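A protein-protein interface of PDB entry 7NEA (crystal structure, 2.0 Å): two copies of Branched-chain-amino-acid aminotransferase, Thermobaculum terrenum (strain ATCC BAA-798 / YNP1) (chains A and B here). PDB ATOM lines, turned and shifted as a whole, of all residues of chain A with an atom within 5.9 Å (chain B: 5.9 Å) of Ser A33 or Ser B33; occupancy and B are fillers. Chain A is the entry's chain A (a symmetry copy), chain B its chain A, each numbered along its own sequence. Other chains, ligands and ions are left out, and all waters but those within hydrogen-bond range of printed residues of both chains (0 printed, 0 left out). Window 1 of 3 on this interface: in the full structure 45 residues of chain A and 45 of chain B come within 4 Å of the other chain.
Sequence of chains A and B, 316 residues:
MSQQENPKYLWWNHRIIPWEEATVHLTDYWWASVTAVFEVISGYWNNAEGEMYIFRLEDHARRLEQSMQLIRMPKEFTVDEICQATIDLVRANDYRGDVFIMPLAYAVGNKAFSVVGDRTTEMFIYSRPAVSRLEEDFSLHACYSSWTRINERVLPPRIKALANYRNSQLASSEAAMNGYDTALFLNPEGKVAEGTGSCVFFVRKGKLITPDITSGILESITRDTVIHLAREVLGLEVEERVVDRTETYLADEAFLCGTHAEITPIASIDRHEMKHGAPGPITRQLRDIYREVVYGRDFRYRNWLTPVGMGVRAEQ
Printed residues of chain B within 4 Å of Trp A31: Leu B162 (3.8 Å).
Ser A33 touches just these residues of chain B: Trp B30 (3.9 Å), Ser B33 (3.4 Å) and Leu B162 (3.9 Å).
Of the printed residues of chain A, Tyr B106 touches Trp A30 (3.5 Å).
The nearest printed residue of chain B that does not touch Ser A33 is Val B34 (5.9 Å).
The nearest printed residue of chain A that does not touch Ser B33 is Val A34 (5.9 Å).
The nearest printed residue of chain A that does not touch Tyr B29 is Ser A33 (6.5 Å).
Trp A30 touches Tyr B106, and with the chains exchanged Tyr A106 touches Trp B30.
Ser A33 touches Leu B162, and with the chains exchanged Leu A162 touches Ser B33.
Val A34 touches Leu B162, and with the chains exchanged Leu A162 touches Val B34.
Ala B163 touches its own counterpart, Ala A163.
12 positions are printed for both chains.
Of the 16 pairs that touch across the chains among the printed residues, 16 have their exchanged pair printed and touching as well.
Printed residues of chain B that touch a printed residue of chain A: Tyr B29, Trp B30, Trp B31, Ser B33, Val B34, Tyr B106, Leu B162 and Ala B163.
Printed residues of chain A that touch a printed residue of chain B: Tyr A29, Trp A30, Trp A31, Ser A33, Val A34, Tyr A106, Leu A162 and Ala A163.
Hydrophobic or aromatic side chains of chain A that line the printed part of chain B: Tyr A29, Trp A30, Trp A31, Val A34, Tyr A106, Leu A162 and Ala A163.
Among the printed residues, no Asp or Glu carboxylate lies within 4 Å of a Lys or Arg side-chain nitrogen of the other chain.
Tyr A29 touches Trp B30.
Trp A30 touches Tyr B29 (CH2 to CB, 3.8 Å).
Trp A30 touches Tyr B106 (CH2 to CG, 3.5 Å).
Leu B162 touches Trp A30 (CD2 to O, 3.7 Å).
CB of Ser A33 touches OG of Ser B33 (3.4 Å).
Ser A33 touches Leu B162.
Val A34 touches Leu B162.
Tyr A106 touches Trp B30 (CG to CH2, 3.5 Å).
Trp B30 touches Leu A162.
O of Leu A162 touches CG2 of Val B34, at 3.4 Å.
O of Trp B30 lies within hydrogen-bond range of OG of Ser B33, at 2.5 Å.
The backbone NH of Leu B162 lies within hydrogen-bond range of the backbone carbonyl oxygen of Ala B36, at 3.1 Å.
O of Trp A30 is in hydrogen-bond range of OG of Ser A33 (2.5 Å).
N of Leu A162 sits at hydrogen-bond distance from O of Ala A36.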
ATOM      1  N   TYR A  29     -11.367  -4.660  13.498  1.00  0.00           N
ATOM      2  CA  TYR A  29     -12.559  -5.179  14.213  1.00  0.00           C
ATOM      3  C   TYR A  29     -12.544  -6.698  14.460  1.00  0.00           C
ATOM      4  O   TYR A  29     -13.425  -7.164  15.230  1.00  0.00           O
ATOM      5  CB  TYR A  29     -13.807  -4.755  13.435  1.00  0.00           C
ATOM      6  CG  TYR A  29     -13.946  -3.268  13.318  1.00  0.00           C
ATOM      7  CD1 TYR A  29     -13.466  -2.406  14.293  1.00  0.00           C
ATOM      8  CD2 TYR A  29     -14.495  -2.716  12.187  1.00  0.00           C
ATOM      9  CE1 TYR A  29     -13.577  -1.026  14.158  1.00  0.00           C
ATOM     10  CE2 TYR A  29     -14.605  -1.352  12.032  1.00  0.00           C
ATOM     11  CZ  TYR A  29     -14.126  -0.494  12.999  1.00  0.00           C
ATOM     12  OH  TYR A  29     -14.329   0.841  12.751  1.00  0.00           O
ATOM     13  N   TRP A  30     -11.568  -7.468  13.921  1.00  0.00           N
ATOM     14  CA  TRP A  30     -11.480  -8.917  14.237  1.00  0.00           C
ATOM     15  C   TRP A  30     -11.529  -9.133  15.750  1.00  0.00           C
ATOM     16  O   TRP A  30     -12.367  -9.956  16.148  1.00  0.00           O
ATOM     17  CB  TRP A  30     -10.318  -9.625  13.548  1.00  0.00           C
ATOM     18  CG  TRP A  30     -10.522  -9.662  12.056  1.00  0.00           C
ATOM     19  CD1 TRP A  30     -10.055  -8.718  11.191  1.00  0.00           C
ATOM     20  CD2 TRP A  30     -11.231 -10.607  11.227  1.00  0.00           C
ATOM     21  NE1 TRP A  30     -10.477  -8.969   9.906  1.00  0.00           N
ATOM     22  CE2 TRP A  30     -11.151 -10.147   9.889  1.00  0.00           C
ATOM     23  CE3 TRP A  30     -11.901 -11.819  11.443  1.00  0.00           C
ATOM     24  CZ2 TRP A  30     -11.650 -10.863   8.799  1.00  0.00           C
ATOM     25  CZ3 TRP A  30     -12.442 -12.502  10.382  1.00  0.00           C
ATOM     26  CH2 TRP A  30     -12.278 -12.060   9.066  1.00  0.00           C
ATOM     27  N   TRP A  31     -10.755  -8.420  16.557  1.00  0.00           N
ATOM     28  CA  TRP A  31     -10.825  -8.545  18.031  1.00  0.00           C
ATOM     29  C   TRP A  31     -12.193  -8.034  18.489  1.00  0.00           C
ATOM     30  O   TRP A  31     -12.737  -8.668  19.351  1.00  0.00           O
ATOM     31  CB  TRP A  31      -9.643  -7.870  18.744  1.00  0.00           C
ATOM     32  CG  TRP A  31      -8.398  -8.686  18.616  1.00  0.00           C
ATOM     33  CD1 TRP A  31      -7.185  -8.335  18.067  1.00  0.00           C
ATOM     34  CD2 TRP A  31      -8.260 -10.034  19.106  1.00  0.00           C
ATOM     35  NE1 TRP A  31      -6.300  -9.377  18.192  1.00  0.00           N
ATOM     36  CE2 TRP A  31      -6.940 -10.439  18.801  1.00  0.00           C
ATOM     37  CE3 TRP A  31      -9.114 -10.904  19.801  1.00  0.00           C
ATOM     38  CZ2 TRP A  31      -6.485 -11.718  19.139  1.00  0.00           C
ATOM     39  CZ3 TRP A  31      -8.662 -12.158  20.151  1.00  0.00           C
ATOM     40  CH2 TRP A  31      -7.372 -12.566  19.780  1.00  0.00           C
ATOM     41  N   ALA A  32     -12.744  -6.978  17.889  1.00  0.00           N
ATOM     42  CA  ALA A  32     -14.078  -6.453  18.299  1.00  0.00           C
ATOM     43  C   ALA A  32     -15.168  -7.500  18.070  1.00  0.00           C
ATOM     44  O   ALA A  32     -16.232  -7.492  18.789  1.00  0.00           O
ATOM     45  CB  ALA A  32     -14.367  -5.198  17.515  1.00  0.00           C
ATOM     46  N   SER A  33     -15.001  -8.365  17.071  1.00  0.00           N
ATOM     47  CA  SER A  33     -16.030  -9.364  16.763  1.00  0.00           C
ATOM     48  C   SER A  33     -16.215 -10.329  17.935  1.00  0.00           C
ATOM     49  O   SER A  33     -17.280 -10.898  17.980  1.00  0.00           O
ATOM     50  CB  SER A  33     -15.770 -10.143  15.499  1.00  0.00           C
ATOM     51  OG  SER A  33     -14.622 -10.986  15.659  1.00  0.00           O
ATOM     52  N   VAL A  34     -15.214 -10.587  18.752  1.00  0.00           N
ATOM     53  CA  VAL A  34     -15.370 -11.471  19.948  1.00  0.00           C
ATOM     54  C   VAL A  34     -16.498 -10.907  20.863  1.00  0.00           C
ATOM     55  O   VAL A  34     -17.164 -11.696  21.481  1.00  0.00           O
ATOM     56  CB  VAL A  34     -14.037 -11.555  20.692  1.00  0.00           C
ATOM     57  CG1 VAL A  34     -14.144 -12.392  21.957  1.00  0.00           C
ATOM     58  CG2 VAL A  34     -12.963 -12.091  19.731  1.00  0.00           C
ATOM     59  N   THR A  35     -16.696  -9.581  20.898  1.00  0.00           N
ATOM     60  CA  THR A  35     -17.655  -8.857  21.778  1.00  0.00           C
ATOM     61  C   THR A  35     -19.014  -8.795  21.119  1.00  0.00           C
ATOM     62  O   THR A  35     -19.966  -8.390  21.821  1.00  0.00           O
ATOM     63  CB  THR A  35     -17.264  -7.380  22.012  1.00  0.00           C
ATOM     64  OG1 THR A  35     -17.484  -6.536  20.822  1.00  0.00           O
ATOM     65  CG2 THR A  35     -15.858  -7.321  22.528  1.00  0.00           C
ATOM     66  N   ALA A  36     -19.102  -9.062  19.816  1.00  0.00           N
ATOM     67  CA  ALA A  36     -20.225  -8.531  19.002  1.00  0.00           C
ATOM     68  C   ALA A  36     -21.518  -9.245  19.364  1.00  0.00           C
ATOM     69  O   ALA A  36     -21.515 -10.483  19.544  1.00  0.00           O
ATOM     70  CB  ALA A  36     -19.963  -8.672  17.517  1.00  0.00           C
ATOM     71  N   TYR A 106     -20.692  -3.759  18.665  1.00  0.00           N
ATOM     72  CA  TYR A 106     -19.307  -4.260  18.881  1.00  0.00           C
ATOM     73  C   TYR A 106     -18.622  -3.189  19.718  1.00  0.00           C
ATOM     74  O   TYR A 106     -18.888  -1.954  19.560  1.00  0.00           O
ATOM     75  CB  TYR A 106     -18.674  -4.657  17.544  1.00  0.00           C
ATOM     76  CG  TYR A 106     -18.554  -3.556  16.534  1.00  0.00           C
ATOM     77  CD1 TYR A 106     -19.565  -3.216  15.646  1.00  0.00           C
ATOM     78  CD2 TYR A 106     -17.397  -2.825  16.461  1.00  0.00           C
ATOM     79  CE1 TYR A 106     -19.398  -2.194  14.717  1.00  0.00           C
ATOM     80  CE2 TYR A 106     -17.253  -1.748  15.594  1.00  0.00           C
ATOM     81  CZ  TYR A 106     -18.275  -1.386  14.730  1.00  0.00           C
ATOM     82  OH  TYR A 106     -18.067  -0.280  13.895  1.00  0.00           O
ATOM     83  N   ALA A 107     -17.699  -3.618  20.569  1.00  0.00           N
ATOM     84  CA  ALA A 107     -16.848  -2.699  21.343  1.00  0.00           C
ATOM     85  C   ALA A 107     -15.426  -2.784  20.808  1.00  0.00           C
ATOM     86  O   ALA A 107     -14.880  -3.908  20.737  1.00  0.00           O
ATOM     87  CB  ALA A 107     -16.952  -3.054  22.794  1.00  0.00           C
ATOM     88  N   LEU A 162     -22.271 -13.266  18.463  1.00  0.00           N
ATOM     89  CA  LEU A 162     -21.678 -13.987  17.337  1.00  0.00           C
ATOM     90  C   LEU A 162     -20.901 -15.207  17.855  1.00  0.00           C
ATOM     91  O   LEU A 162     -20.955 -16.260  17.223  1.00  0.00           O
ATOM     92  CB  LEU A 162     -20.694 -13.050  16.626  1.00  0.00           C
ATOM     93  CG  LEU A 162     -21.004 -12.513  15.253  1.00  0.00           C
ATOM     94  CD1 LEU A 162     -22.449 -12.395  14.904  1.00  0.00           C
ATOM     95  CD2 LEU A 162     -20.158 -11.277  14.945  1.00  0.00           C
ATOM     96  N   ALA A 163     -20.144 -15.069  18.932  1.00  0.00           N
ATOM     97  CA  ALA A 163     -19.240 -16.121  19.418  1.00  0.00           C
ATOM     98  C   ALA A 163     -20.032 -17.405  19.731  1.00  0.00           C
ATOM     99  O   ALA A 163     -19.471 -18.496  19.591  1.00  0.00           O
ATOM    100  CB  ALA A 163     -18.450 -15.660  20.606  1.00  0.00           C
ATOM    101  N   TYR B  29     -17.559 -10.159   6.495  1.00  0.00           N
ATOM    102  CA  TYR B  29     -16.783 -11.125   7.311  1.00  0.00           C
ATOM    103  C   TYR B  29     -17.260 -11.255   8.769  1.00  0.00           C
ATOM    104  O   TYR B  29     -16.773 -12.195   9.451  1.00  0.00           O
ATOM    105  CB  TYR B  29     -15.305 -10.729   7.245  1.00  0.00           C
ATOM    106  CG  TYR B  29     -14.756 -10.755   5.851  1.00  0.00           C
ATOM    107  CD1 TYR B  29     -15.238 -11.627   4.887  1.00  0.00           C
ATOM    108  CD2 TYR B  29     -13.798  -9.847   5.475  1.00  0.00           C
ATOM    109  CE1 TYR B  29     -14.739 -11.619   3.589  1.00  0.00           C
ATOM    110  CE2 TYR B  29     -13.298  -9.819   4.191  1.00  0.00           C
ATOM    111  CZ  TYR B  29     -13.779 -10.684   3.231  1.00  0.00           C
ATOM    112  OH  TYR B  29     -13.174 -10.588   2.001  1.00  0.00           O
ATOM    113  N   TRP B  30     -18.220 -10.428   9.250  1.00  0.00           N
ATOM    114  CA  TRP B  30     -18.765 -10.611  10.620  1.00  0.00           C
ATOM    115  C   TRP B  30     -19.185 -12.066  10.834  1.00  0.00           C
ATOM    116  O   TRP B  30     -18.731 -12.613  11.849  1.00  0.00           O
ATOM    117  CB  TRP B  30     -19.841  -9.596  10.991  1.00  0.00           C
ATOM    118  CG  TRP B  30     -19.259  -8.211  11.089  1.00  0.00           C
ATOM    119  CD1 TRP B  30     -19.211  -7.319  10.060  1.00  0.00           C
ATOM    120  CD2 TRP B  30     -18.625  -7.533  12.196  1.00  0.00           C
ATOM    121  NE1 TRP B  30     -18.539  -6.176  10.423  1.00  0.00           N
ATOM    122  CE2 TRP B  30     -18.218  -6.255  11.739  1.00  0.00           C
ATOM    123  CE3 TRP B  30     -18.380  -7.834  13.542  1.00  0.00           C
ATOM    124  CZ2 TRP B  30     -17.648  -5.288  12.568  1.00  0.00           C
ATOM    125  CZ3 TRP B  30     -17.771  -6.908  14.352  1.00  0.00           C
ATOM    126  CH2 TRP B  30     -17.451  -5.628  13.889  1.00  0.00           C
ATOM    127  N   TRP B  31     -19.934 -12.690   9.932  1.00  0.00           N
ATOM    128  CA  TRP B  31     -20.300 -14.118  10.065  1.00  0.00           C
ATOM    129  C   TRP B  31     -19.021 -14.952   9.939  1.00  0.00           C
ATOM    130  O   TRP B  31     -18.916 -15.881  10.692  1.00  0.00           O
ATOM    131  CB  TRP B  31     -21.411 -14.542   9.092  1.00  0.00           C
ATOM    132  CG  TRP B  31     -22.744 -14.039   9.542  1.00  0.00           C
ATOM    133  CD1 TRP B  31     -23.628 -13.217   8.881  1.00  0.00           C
ATOM    134  CD2 TRP B  31     -23.355 -14.382  10.800  1.00  0.00           C
ATOM    135  NE1 TRP B  31     -24.754 -13.035   9.644  1.00  0.00           N
ATOM    136  CE2 TRP B  31     -24.603 -13.716  10.835  1.00  0.00           C
ATOM    137  CE3 TRP B  31     -22.979 -15.216  11.865  1.00  0.00           C
ATOM    138  CZ2 TRP B  31     -25.449 -13.836  11.942  1.00  0.00           C
ATOM    139  CZ3 TRP B  31     -23.820 -15.349  12.949  1.00  0.00           C
ATOM    140  CH2 TRP B  31     -25.022 -14.627  12.995  1.00  0.00           C
ATOM    141  N   ALA B  32     -18.073 -14.591   9.074  1.00  0.00           N
ATOM    142  CA  ALA B  32     -16.810 -15.368   8.927  1.00  0.00           C
ATOM    143  C   ALA B  32     -16.012 -15.362  10.231  1.00  0.00           C
ATOM    144  O   ALA B  32     -15.218 -16.332  10.507  1.00  0.00           O
ATOM    145  CB  ALA B  32     -16.003 -14.775   7.801  1.00  0.00           C
ATOM    146  N   SER B  33     -16.123 -14.298  11.024  1.00  0.00           N
ATOM    147  CA  SER B  33     -15.348 -14.202  12.265  1.00  0.00           C
ATOM    148  C   SER B  33     -15.744 -15.313  13.238  1.00  0.00           C
ATOM    149  O   SER B  33     -14.918 -15.596  14.073  1.00  0.00           O
ATOM    150  CB  SER B  33     -15.451 -12.865  12.952  1.00  0.00           C
ATOM    151  OG  SER B  33     -16.778 -12.661  13.453  1.00  0.00           O
ATOM    152  N   VAL B  34     -16.959 -15.821  13.211  1.00  0.00           N
ATOM    153  CA  VAL B  34     -17.369 -16.953  14.098  1.00  0.00           C
ATOM    154  C   VAL B  34     -16.424 -18.168  13.855  1.00  0.00           C
ATOM    155  O   VAL B  34     -16.179 -18.883  14.791  1.00  0.00           O
ATOM    156  CB  VAL B  34     -18.827 -17.316  13.816  1.00  0.00           C
ATOM    157  CG1 VAL B  34     -19.289 -18.505  14.644  1.00  0.00           C
ATOM    158  CG2 VAL B  34     -19.703 -16.073  14.048  1.00  0.00           C
ATOM    159  N   THR B  35     -15.903 -18.343  12.632  1.00  0.00           N
ATOM    160  CA  THR B  35     -15.063 -19.489  12.189  1.00  0.00           C
ATOM    161  C   THR B  35     -13.609 -19.215  12.500  1.00  0.00           C
ATOM    162  O   THR B  35     -12.810 -20.167  12.363  1.00  0.00           O
ATOM    163  CB  THR B  35     -15.102 -19.714  10.661  1.00  0.00           C
ATOM    164  OG1 THR B  35     -14.356 -18.683   9.913  1.00  0.00           O
ATOM    165  CG2 THR B  35     -16.529 -19.847  10.221  1.00  0.00           C
ATOM    166  N   ALA B  36     -13.245 -17.965  12.788  1.00  0.00           N
ATOM    167  CA  ALA B  36     -11.847 -17.511  12.583  1.00  0.00           C
ATOM    168  C   ALA B  36     -10.933 -18.149  13.618  1.00  0.00           C
ATOM    169  O   ALA B  36     -11.307 -18.236  14.809  1.00  0.00           O
ATOM    170  CB  ALA B  36     -11.725 -16.003  12.657  1.00  0.00           C
ATOM    171  N   TYR B 106     -10.076 -17.633   8.116  1.00  0.00           N
ATOM    172  CA  TYR B 106     -11.548 -17.445   8.224  1.00  0.00           C
ATOM    173  C   TYR B 106     -12.129 -18.144   7.004  1.00  0.00           C
ATOM    174  O   TYR B 106     -11.518 -18.145   5.887  1.00  0.00           O
ATOM    175  CB  TYR B 106     -11.878 -15.964   8.442  1.00  0.00           C
ATOM    176  CG  TYR B 106     -11.429 -15.036   7.354  1.00  0.00           C
ATOM    177  CD1 TYR B 106     -10.163 -14.467   7.305  1.00  0.00           C
ATOM    178  CD2 TYR B 106     -12.290 -14.712   6.340  1.00  0.00           C
ATOM    179  CE1 TYR B 106      -9.800 -13.599   6.280  1.00  0.00           C
ATOM    180  CE2 TYR B 106     -11.909 -13.913   5.268  1.00  0.00           C
ATOM    181  CZ  TYR B 106     -10.633 -13.373   5.199  1.00  0.00           C
ATOM    182  OH  TYR B 106     -10.311 -12.590   4.083  1.00  0.00           O
ATOM    183  N   ALA B 107     -13.327 -18.693   7.163  1.00  0.00           N
ATOM    184  CA  ALA B 107     -14.084 -19.279   6.044  1.00  0.00           C
ATOM    185  C   ALA B 107     -15.280 -18.387   5.745  1.00  0.00           C
ATOM    186  O   ALA B 107     -16.060 -18.099   6.680  1.00  0.00           O
ATOM    187  CB  ALA B 107     -14.472 -20.679   6.406  1.00  0.00           C
ATOM    188  N   LEU B 162     -11.042 -17.205  17.697  1.00  0.00           N
ATOM    189  CA  LEU B 162     -11.476 -15.916  18.237  1.00  0.00           C
ATOM    190  C   LEU B 162     -12.655 -16.129  19.200  1.00  0.00           C
ATOM    191  O   LEU B 162     -12.708 -15.463  20.232  1.00  0.00           O
ATOM    192  CB  LEU B 162     -11.951 -15.038  17.073  1.00  0.00           C
ATOM    193  CG  LEU B 162     -11.153 -13.834  16.648  1.00  0.00           C
ATOM    194  CD1 LEU B 162      -9.689 -13.883  16.926  1.00  0.00           C
ATOM    195  CD2 LEU B 162     -11.531 -13.400  15.231  1.00  0.00           C
ATOM    196  N   ALA B 163     -13.610 -16.978  18.857  1.00  0.00           N
ATOM    197  CA  ALA B 163     -14.854 -17.137  19.623  1.00  0.00           C
ATOM    198  C   ALA B 163     -14.540 -17.560  21.073  1.00  0.00           C
ATOM    199  O   ALA B 163     -15.308 -17.204  21.972  1.00  0.00           O
ATOM    200  CB  ALA B 163     -15.787 -18.106  18.960  1.00  0.00           C
